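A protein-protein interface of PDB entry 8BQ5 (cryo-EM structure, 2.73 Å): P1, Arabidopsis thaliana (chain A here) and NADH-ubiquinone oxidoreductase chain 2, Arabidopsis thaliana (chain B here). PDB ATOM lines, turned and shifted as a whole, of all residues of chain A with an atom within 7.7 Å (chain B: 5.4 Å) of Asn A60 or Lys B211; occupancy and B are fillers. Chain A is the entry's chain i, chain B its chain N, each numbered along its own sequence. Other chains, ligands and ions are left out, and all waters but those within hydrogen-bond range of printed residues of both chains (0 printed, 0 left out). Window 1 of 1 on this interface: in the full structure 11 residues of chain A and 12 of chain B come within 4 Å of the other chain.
Printed residues of chain B that touch a printed residue of chain A: Asp B207, Gln B208, Lys B211 and Thr B214.
Of the 15 printed residues of chain A, 6 touch a printed residue of chain B.
Printed residues of chain A that touch a printed residue of chain B: Phe A53, Trp A54, Arg A58, His A59, Asn A60 and Gln A62.
Along chain A the printed residues that touch a printed residue of chain B span positions 53 to 62.
Among the printed residues, 8 pairs touch across the chains.
Among the printed residues, pairs that only touch across the chains: Phe A53 with Thr B214, Trp A54 with Lys B211, Trp A54 with Thr B214, Arg A58 with Asp B207 and Asn A60 with Lys B211.
Of chain B, only Lys B211 (3.8 Å) comes within 4 Å of Asn A60.
No residue of chain A comes within 4 Å of Ala B210.
Of the printed residues of chain A, Thr B214 touches Phe A53 and Trp A54.
Of the printed residues of chain A, Asp B207 touches Arg A58 and His A59.
Of the printed residues of chain B, Trp A54 touches Lys B211 and Thr B214.
Of the printed residues of chain A, Gln B208 touches Gln A62 (3.0 Å).
Phe A56 touches none of the printed residues of chain B.
The nearest residue of chain B that does not touch Asn A60 is Asp B207 (4.1 Å).
The nearest printed residue of chain A that does not touch Asp B207 is Asn A60 (4.1 Å).
The side-chain amide nitrogen (ND2) of Asn A60 sits at hydrogen-bond distance from the backbone carbonyl oxygen (O) of Phe A56.
The backbone carbonyl oxygen (O) of Ala B210 sits at hydrogen-bond distance from the side-chain hydroxyl (OG1) of Thr B214 (2.9 Å).
The backbone carbonyl oxygen (O) of Lys B211 lies within hydrogen-bond range of the side-chain hydroxyl (OG1) of Thr B214, 2.9 Å away.
The backbone carbonyl oxygen (O) of Trp A54 lies within hydrogen-bond range of the side-chain amide nitrogen (ND2) of Asn A60 (2.8 Å).
The side-chain carboxylate (OD2) of Asp A66 is in hydrogen-bond range of the side-chain amide nitrogen (NE2) of Gln A62, at 2.8 Å.
The backbone carbonyl oxygen of Phe A53 sits at hydrogen-bond distance from a ring nitrogen (ND1) of His A59.
O of His A59 sits close to OD2 of Asp B207 (3.4 Å).
The side-chain amino group of Lys B211 sits at hydrogen-bond distance from the backbone carbonyl oxygen of His A59, 2.9 Å away.
The side-chain amide nitrogen (NE2) of Gln B208 lies within hydrogen-bond range of the side-chain amide oxygen (OE1) of Gln A62.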
ATOM      1  N   GLY A  52      -8.309 -21.457  26.904  1.00  0.00           N
ATOM      2  CA  GLY A  52      -7.629 -21.466  25.624  1.00  0.00           C
ATOM      3  C   GLY A  52      -8.527 -21.862  24.472  1.00  0.00           C
ATOM      4  O   GLY A  52      -8.261 -22.850  23.782  1.00  0.00           O
ATOM      5  N   PHE A  53      -9.608 -21.108  24.269  1.00  0.00           N
ATOM      6  CA  PHE A  53     -10.533 -21.410  23.181  1.00  0.00           C
ATOM      7  C   PHE A  53      -9.852 -21.313  21.821  1.00  0.00           C
ATOM      8  O   PHE A  53     -10.286 -21.952  20.856  1.00  0.00           O
ATOM      9  CB  PHE A  53     -11.740 -20.477  23.251  1.00  0.00           C
ATOM     10  CG  PHE A  53     -11.488 -19.116  22.673  1.00  0.00           C
ATOM     11  CD1 PHE A  53     -10.469 -18.319  23.168  1.00  0.00           C
ATOM     12  CD2 PHE A  53     -12.266 -18.629  21.642  1.00  0.00           C
ATOM     13  CE1 PHE A  53     -10.231 -17.069  22.644  1.00  0.00           C
ATOM     14  CE2 PHE A  53     -12.032 -17.376  21.118  1.00  0.00           C
ATOM     15  CZ  PHE A  53     -11.013 -16.596  21.618  1.00  0.00           C
ATOM     16  N   TRP A  54      -8.780 -20.521  21.725  1.00  0.00           N
ATOM     17  CA  TRP A  54      -8.026 -20.425  20.481  1.00  0.00           C
ATOM     18  C   TRP A  54      -7.358 -21.742  20.103  1.00  0.00           C
ATOM     19  O   TRP A  54      -6.951 -21.900  18.946  1.00  0.00           O
ATOM     20  CB  TRP A  54      -6.985 -19.308  20.596  1.00  0.00           C
ATOM     21  CG  TRP A  54      -6.048 -19.507  21.737  1.00  0.00           C
ATOM     22  CD1 TRP A  54      -4.879 -20.195  21.718  1.00  0.00           C
ATOM     23  CD2 TRP A  54      -6.207 -19.021  23.076  1.00  0.00           C
ATOM     24  NE1 TRP A  54      -4.293 -20.172  22.960  1.00  0.00           N
ATOM     25  CE2 TRP A  54      -5.090 -19.455  23.812  1.00  0.00           C
ATOM     26  CE3 TRP A  54      -7.186 -18.261  23.722  1.00  0.00           C
ATOM     27  CZ2 TRP A  54      -4.922 -19.154  25.160  1.00  0.00           C
ATOM     28  CZ3 TRP A  54      -7.019 -17.962  25.058  1.00  0.00           C
ATOM     29  CH2 TRP A  54      -5.895 -18.408  25.764  1.00  0.00           C
ATOM     30  N   THR A  55      -7.245 -22.685  21.044  1.00  0.00           N
ATOM     31  CA  THR A  55      -6.694 -24.004  20.748  1.00  0.00           C
ATOM     32  C   THR A  55      -7.682 -24.877  19.978  1.00  0.00           C
ATOM     33  O   THR A  55      -7.271 -25.826  19.300  1.00  0.00           O
ATOM     34  CB  THR A  55      -6.285 -24.694  22.055  1.00  0.00           C
ATOM     35  OG1 THR A  55      -5.508 -23.793  22.852  1.00  0.00           O
ATOM     36  CG2 THR A  55      -5.472 -25.952  21.793  1.00  0.00           C
ATOM     37  N   PHE A  56      -8.984 -24.578  20.111  1.00  0.00           N
ATOM     38  CA  PHE A  56     -10.037 -25.406  19.461  1.00  0.00           C
ATOM     39  C   PHE A  56      -9.819 -25.448  17.947  1.00  0.00           C
ATOM     40  O   PHE A  56      -9.391 -24.432  17.370  1.00  0.00           O
ATOM     41  CB  PHE A  56     -11.449 -24.927  19.801  1.00  0.00           C
ATOM     42  CG  PHE A  56     -11.797 -24.849  21.269  1.00  0.00           C
ATOM     43  CD1 PHE A  56     -11.075 -25.548  22.224  1.00  0.00           C
ATOM     44  CD2 PHE A  56     -12.861 -24.072  21.694  1.00  0.00           C
ATOM     45  CE1 PHE A  56     -11.400 -25.460  23.568  1.00  0.00           C
ATOM     46  CE2 PHE A  56     -13.191 -23.991  23.037  1.00  0.00           C
ATOM     47  CZ  PHE A  56     -12.459 -24.683  23.973  1.00  0.00           C
ATOM     48  N   GLU A  57     -10.176 -26.568  17.318  1.00  0.00           N
ATOM     49  CA  GLU A  57      -9.873 -26.780  15.905  1.00  0.00           C
ATOM     50  C   GLU A  57     -10.603 -25.800  14.995  1.00  0.00           C
ATOM     51  O   GLU A  57     -10.078 -25.428  13.941  1.00  0.00           O
ATOM     52  CB  GLU A  57     -10.209 -28.219  15.505  1.00  0.00           C
ATOM     53  CG  GLU A  57      -9.174 -29.248  15.947  1.00  0.00           C
ATOM     54  CD  GLU A  57      -9.102 -29.406  17.453  1.00  0.00           C
ATOM     55  OE1 GLU A  57     -10.080 -29.040  18.140  1.00  0.00           O
ATOM     56  OE2 GLU A  57      -8.063 -29.887  17.953  1.00  0.00           O
ATOM     57  N   ARG A  58     -11.812 -25.377  15.378  1.00  0.00           N
ATOM     58  CA  ARG A  58     -12.529 -24.381  14.586  1.00  0.00           C
ATOM     59  C   ARG A  58     -11.746 -23.079  14.484  1.00  0.00           C
ATOM     60  O   ARG A  58     -11.853 -22.365  13.480  1.00  0.00           O
ATOM     61  CB  ARG A  58     -13.913 -24.130  15.192  1.00  0.00           C
ATOM     62  CG  ARG A  58     -14.660 -22.920  14.629  1.00  0.00           C
ATOM     63  CD  ARG A  58     -15.110 -23.129  13.188  1.00  0.00           C
ATOM     64  NE  ARG A  58     -14.114 -22.674  12.226  1.00  0.00           N
ATOM     65  CZ  ARG A  58     -14.183 -22.877  10.917  1.00  0.00           C
ATOM     66  NH1 ARG A  58     -15.207 -23.507  10.366  1.00  0.00           N
ATOM     67  NH2 ARG A  58     -13.197 -22.436  10.139  1.00  0.00           N
ATOM     68  N   HIS A  59     -10.911 -22.776  15.490  1.00  0.00           N
ATOM     69  CA  HIS A  59     -10.177 -21.480  15.523  1.00  0.00           C
ATOM     70  C   HIS A  59      -8.762 -21.643  14.963  1.00  0.00           C
ATOM     71  O   HIS A  59      -7.931 -20.760  15.230  1.00  0.00           O
ATOM     72  CB  HIS A  59     -10.147 -20.903  16.942  1.00  0.00           C
ATOM     73  CG  HIS A  59     -11.447 -20.948  17.671  1.00  0.00           C
ATOM     74  ND1 HIS A  59     -12.067 -22.129  18.022  1.00  0.00           N
ATOM     75  CD2 HIS A  59     -12.230 -19.960  18.146  1.00  0.00           C
ATOM     76  CE1 HIS A  59     -13.188 -21.868  18.655  1.00  0.00           C
ATOM     77  NE2 HIS A  59     -13.307 -20.547  18.751  1.00  0.00           N
ATOM     78  N   ASN A  60      -8.508 -22.711  14.210  1.00  0.00           N
ATOM     79  CA  ASN A  60      -7.184 -22.988  13.658  1.00  0.00           C
ATOM     80  C   ASN A  60      -7.226 -23.165  12.149  1.00  0.00           C
ATOM     81  O   ASN A  60      -6.447 -23.932  11.576  1.00  0.00           O
ATOM     82  CB  ASN A  60      -6.593 -24.222  14.324  1.00  0.00           C
ATOM     83  CG  ASN A  60      -5.733 -23.877  15.508  1.00  0.00           C
ATOM     84  OD1 ASN A  60      -4.533 -24.131  15.504  1.00  0.00           O
ATOM     85  ND2 ASN A  60      -6.337 -23.281  16.530  1.00  0.00           N
ATOM     86  N   ALA A  61      -8.142 -22.461  11.486  1.00  0.00           N
ATOM     87  CA  ALA A  61      -8.345 -22.666  10.057  1.00  0.00           C
ATOM     88  C   ALA A  61      -7.127 -22.244   9.242  1.00  0.00           C
ATOM     89  O   ALA A  61      -6.739 -22.940   8.296  1.00  0.00           O
ATOM     90  CB  ALA A  61      -9.591 -21.915   9.600  1.00  0.00           C
ATOM     91  N   GLN A  62      -6.510 -21.107   9.583  1.00  0.00           N
ATOM     92  CA  GLN A  62      -5.362 -20.643   8.804  1.00  0.00           C
ATOM     93  C   GLN A  62      -4.201 -21.623   8.908  1.00  0.00           C
ATOM     94  O   GLN A  62      -3.483 -21.851   7.928  1.00  0.00           O
ATOM     95  CB  GLN A  62      -4.927 -19.245   9.253  1.00  0.00           C
ATOM     96  CG  GLN A  62      -3.579 -18.805   8.670  1.00  0.00           C
ATOM     97  CD  GLN A  62      -3.272 -17.332   8.885  1.00  0.00           C
ATOM     98  OE1 GLN A  62      -3.623 -16.753   9.910  1.00  0.00           O
ATOM     99  NE2 GLN A  62      -2.606 -16.722   7.911  1.00  0.00           N
ATOM    100  N   LEU A  63      -4.018 -22.225  10.083  1.00  0.00           N
ATOM    101  CA  LEU A  63      -2.954 -23.201  10.280  1.00  0.00           C
ATOM    102  C   LEU A  63      -3.113 -24.433   9.401  1.00  0.00           C
ATOM    103  O   LEU A  63      -2.116 -25.104   9.116  1.00  0.00           O
ATOM    104  CB  LEU A  63      -2.898 -23.611  11.750  1.00  0.00           C
ATOM    105  CG  LEU A  63      -1.797 -22.886  12.514  1.00  0.00           C
ATOM    106  CD1 LEU A  63      -2.081 -22.849  13.998  1.00  0.00           C
ATOM    107  CD2 LEU A  63      -0.490 -23.583  12.228  1.00  0.00           C
ATOM    108  N   ARG A  64      -4.332 -24.753   8.969  1.00  0.00           N
ATOM    109  CA  ARG A  64      -4.536 -25.877   8.065  1.00  0.00           C
ATOM    110  C   ARG A  64      -4.718 -25.460   6.612  1.00  0.00           C
ATOM    111  O   ARG A  64      -4.424 -26.259   5.718  1.00  0.00           O
ATOM    112  CB  ARG A  64      -5.750 -26.710   8.501  1.00  0.00           C
ATOM    113  CG  ARG A  64      -5.959 -26.780  10.005  1.00  0.00           C
ATOM    114  CD  ARG A  64      -6.621 -28.089  10.430  1.00  0.00           C
ATOM    115  NE  ARG A  64      -8.065 -28.097  10.224  1.00  0.00           N
ATOM    116  CZ  ARG A  64      -8.692 -28.841   9.323  1.00  0.00           C
ATOM    117  NH1 ARG A  64      -8.027 -29.638   8.501  1.00  0.00           N
ATOM    118  NH2 ARG A  64     -10.018 -28.789   9.247  1.00  0.00           N
ATOM    119  N   TRP A  65      -5.180 -24.236   6.354  1.00  0.00           N
ATOM    120  CA  TRP A  65      -5.423 -23.809   4.980  1.00  0.00           C
ATOM    121  C   TRP A  65      -4.151 -23.288   4.320  1.00  0.00           C
ATOM    122  O   TRP A  65      -3.813 -23.699   3.207  1.00  0.00           O
ATOM    123  CB  TRP A  65      -6.519 -22.742   4.948  1.00  0.00           C
ATOM    124  CG  TRP A  65      -6.707 -22.112   3.603  1.00  0.00           C
ATOM    125  CD1 TRP A  65      -6.505 -20.803   3.275  1.00  0.00           C
ATOM    126  CD2 TRP A  65      -7.128 -22.766   2.400  1.00  0.00           C
ATOM    127  NE1 TRP A  65      -6.780 -20.601   1.945  1.00  0.00           N
ATOM    128  CE2 TRP A  65      -7.162 -21.790   1.385  1.00  0.00           C
ATOM    129  CE3 TRP A  65      -7.473 -24.082   2.081  1.00  0.00           C
ATOM    130  CZ2 TRP A  65      -7.530 -22.090   0.078  1.00  0.00           C
ATOM    131  CZ3 TRP A  65      -7.840 -24.375   0.782  1.00  0.00           C
ATOM    132  CH2 TRP A  65      -7.866 -23.384  -0.203  1.00  0.00           C
ATOM    133  N   ASP A  66      -3.434 -22.396   4.999  1.00  0.00           N
ATOM    134  CA  ASP A  66      -2.267 -21.746   4.406  1.00  0.00           C
ATOM    135  C   ASP A  66      -1.210 -22.703   3.863  1.00  0.00           C
ATOM    136  O   ASP A  66      -0.641 -22.401   2.800  1.00  0.00           O
ATOM    137  CB  ASP A  66      -1.641 -20.785   5.427  1.00  0.00           C
ATOM    138  CG  ASP A  66      -2.229 -19.389   5.349  1.00  0.00           C
ATOM    139  OD1 ASP A  66      -3.260 -19.213   4.670  1.00  0.00           O
ATOM    140  OD2 ASP A  66      -1.654 -18.465   5.961  1.00  0.00           O
ATOM    141  N   PHE B 206     -10.983 -12.496  11.981  1.00  0.00           N
ATOM    142  CA  PHE B 206     -11.388 -12.501  13.386  1.00  0.00           C
ATOM    143  C   PHE B 206     -10.578 -13.496  14.210  1.00  0.00           C
ATOM    144  O   PHE B 206     -10.346 -13.272  15.402  1.00  0.00           O
ATOM    145  CB  PHE B 206     -12.885 -12.796  13.520  1.00  0.00           C
ATOM    146  CG  PHE B 206     -13.771 -11.652  13.114  1.00  0.00           C
ATOM    147  CD1 PHE B 206     -13.232 -10.431  12.742  1.00  0.00           C
ATOM    148  CD2 PHE B 206     -15.149 -11.788  13.137  1.00  0.00           C
ATOM    149  CE1 PHE B 206     -14.046  -9.381  12.375  1.00  0.00           C
ATOM    150  CE2 PHE B 206     -15.968 -10.740  12.773  1.00  0.00           C
ATOM    151  CZ  PHE B 206     -15.415  -9.535  12.389  1.00  0.00           C
ATOM    152  N   ASP B 207     -10.149 -14.604  13.604  1.00  0.00           N
ATOM    153  CA  ASP B 207      -9.312 -15.560  14.327  1.00  0.00           C
ATOM    154  C   ASP B 207      -7.949 -14.962  14.654  1.00  0.00           C
ATOM    155  O   ASP B 207      -7.460 -15.073  15.788  1.00  0.00           O
ATOM    156  CB  ASP B 207      -9.151 -16.841  13.509  1.00  0.00           C
ATOM    157  CG  ASP B 207     -10.191 -17.884  13.848  1.00  0.00           C
ATOM    158  OD1 ASP B 207     -11.106 -17.577  14.640  1.00  0.00           O
ATOM    159  OD2 ASP B 207     -10.096 -19.009  13.317  1.00  0.00           O
ATOM    160  N   GLN B 208      -7.319 -14.321  13.666  1.00  0.00           N
ATOM    161  CA  GLN B 208      -6.025 -13.691  13.897  1.00  0.00           C
ATOM    162  C   GLN B 208      -6.134 -12.611  14.964  1.00  0.00           C
ATOM    163  O   GLN B 208      -5.255 -12.487  15.825  1.00  0.00           O
ATOM    164  CB  GLN B 208      -5.479 -13.105  12.595  1.00  0.00           C
ATOM    165  CG  GLN B 208      -5.472 -14.066  11.415  1.00  0.00           C
ATOM    166  CD  GLN B 208      -5.263 -13.353  10.091  1.00  0.00           C
ATOM    167  OE1 GLN B 208      -5.542 -12.162   9.965  1.00  0.00           O
ATOM    168  NE2 GLN B 208      -4.758 -14.079   9.101  1.00  0.00           N
ATOM    169  N   LEU B 209      -7.210 -11.824  14.925  1.00  0.00           N
ATOM    170  CA  LEU B 209      -7.438 -10.819  15.956  1.00  0.00           C
ATOM    171  C   LEU B 209      -7.646 -11.462  17.319  1.00  0.00           C
ATOM    172  O   LEU B 209      -7.190 -10.935  18.339  1.00  0.00           O
ATOM    173  CB  LEU B 209      -8.638  -9.952  15.581  1.00  0.00           C
ATOM    174  CG  LEU B 209      -8.428  -8.975  14.425  1.00  0.00           C
ATOM    175  CD1 LEU B 209      -9.459  -7.861  14.474  1.00  0.00           C
ATOM    176  CD2 LEU B 209      -7.025  -8.401  14.481  1.00  0.00           C
ATOM    177  N   ALA B 210      -8.344 -12.597  17.361  1.00  0.00           N
ATOM    178  CA  ALA B 210      -8.567 -13.281  18.629  1.00  0.00           C
ATOM    179  C   ALA B 210      -7.248 -13.733  19.243  1.00  0.00           C
ATOM    180  O   ALA B 210      -7.028 -13.578  20.448  1.00  0.00           O
ATOM    181  CB  ALA B 210      -9.509 -14.469  18.427  1.00  0.00           C
ATOM    182  N   LYS B 211      -6.349 -14.283  18.422  1.00  0.00           N
ATOM    183  CA  LYS B 211      -5.071 -14.752  18.953  1.00  0.00           C
ATOM    184  C   LYS B 211      -4.204 -13.597  19.444  1.00  0.00           C
ATOM    185  O   LYS B 211      -3.652 -13.656  20.550  1.00  0.00           O
ATOM    186  CB  LYS B 211      -4.317 -15.553  17.896  1.00  0.00           C
ATOM    187  CG  LYS B 211      -4.741 -16.998  17.770  1.00  0.00           C
ATOM    188  CD  LYS B 211      -4.182 -17.581  16.487  1.00  0.00           C
ATOM    189  CE  LYS B 211      -4.244 -19.092  16.482  1.00  0.00           C
ATOM    190  NZ  LYS B 211      -5.649 -19.572  16.519  1.00  0.00           N
ATOM    191  N   ILE B 212      -4.068 -12.541  18.639  1.00  0.00           N
ATOM    192  CA  ILE B 212      -3.165 -11.445  18.983  1.00  0.00           C
ATOM    193  C   ILE B 212      -3.613 -10.758  20.267  1.00  0.00           C
ATOM    194  O   ILE B 212      -2.792 -10.422  21.129  1.00  0.00           O
ATOM    195  CB  ILE B 212      -3.059 -10.439  17.820  1.00  0.00           C
ATOM    196  CG1 ILE B 212      -2.221 -11.013  16.683  1.00  0.00           C
ATOM    197  CG2 ILE B 212      -2.453  -9.126  18.289  1.00  0.00           C
ATOM    198  CD1 ILE B 212      -2.613 -10.493  15.316  1.00  0.00           C
ATOM    199  N   LEU B 213      -4.920 -10.546  20.420  1.00  0.00           N
ATOM    200  CA  LEU B 213      -5.410  -9.736  21.575  1.00  0.00           C
ATOM    201  C   LEU B 213      -5.501 -10.547  22.865  1.00  0.00           C
ATOM    202  O   LEU B 213      -5.355  -9.933  23.931  1.00  0.00           O
ATOM    203  CB  LEU B 213      -6.789  -9.169  21.229  1.00  0.00           C
ATOM    204  CG  LEU B 213      -6.841  -8.205  20.045  1.00  0.00           C
ATOM    205  CD1 LEU B 213      -8.149  -7.431  20.047  1.00  0.00           C
ATOM    206  CD2 LEU B 213      -5.661  -7.250  20.070  1.00  0.00           C
ATOM    207  N   THR B 214      -5.730 -11.859  22.779  1.00  0.00           N
ATOM    208  CA  THR B 214      -5.957 -12.662  24.010  1.00  0.00           C
ATOM    209  C   THR B 214      -4.757 -12.677  24.943  1.00  0.00           C
ATOM    210  O   THR B 214      -3.629 -12.804  24.448  1.00  0.00           O
ATOM    211  CB  THR B 214      -6.251 -14.142  23.741  1.00  0.00           C
ATOM    212  OG1 THR B 214      -5.408 -14.601  22.683  1.00  0.00           O
ATOM    213  CG2 THR B 214      -7.700 -14.404  23.394  1.00  0.00           C
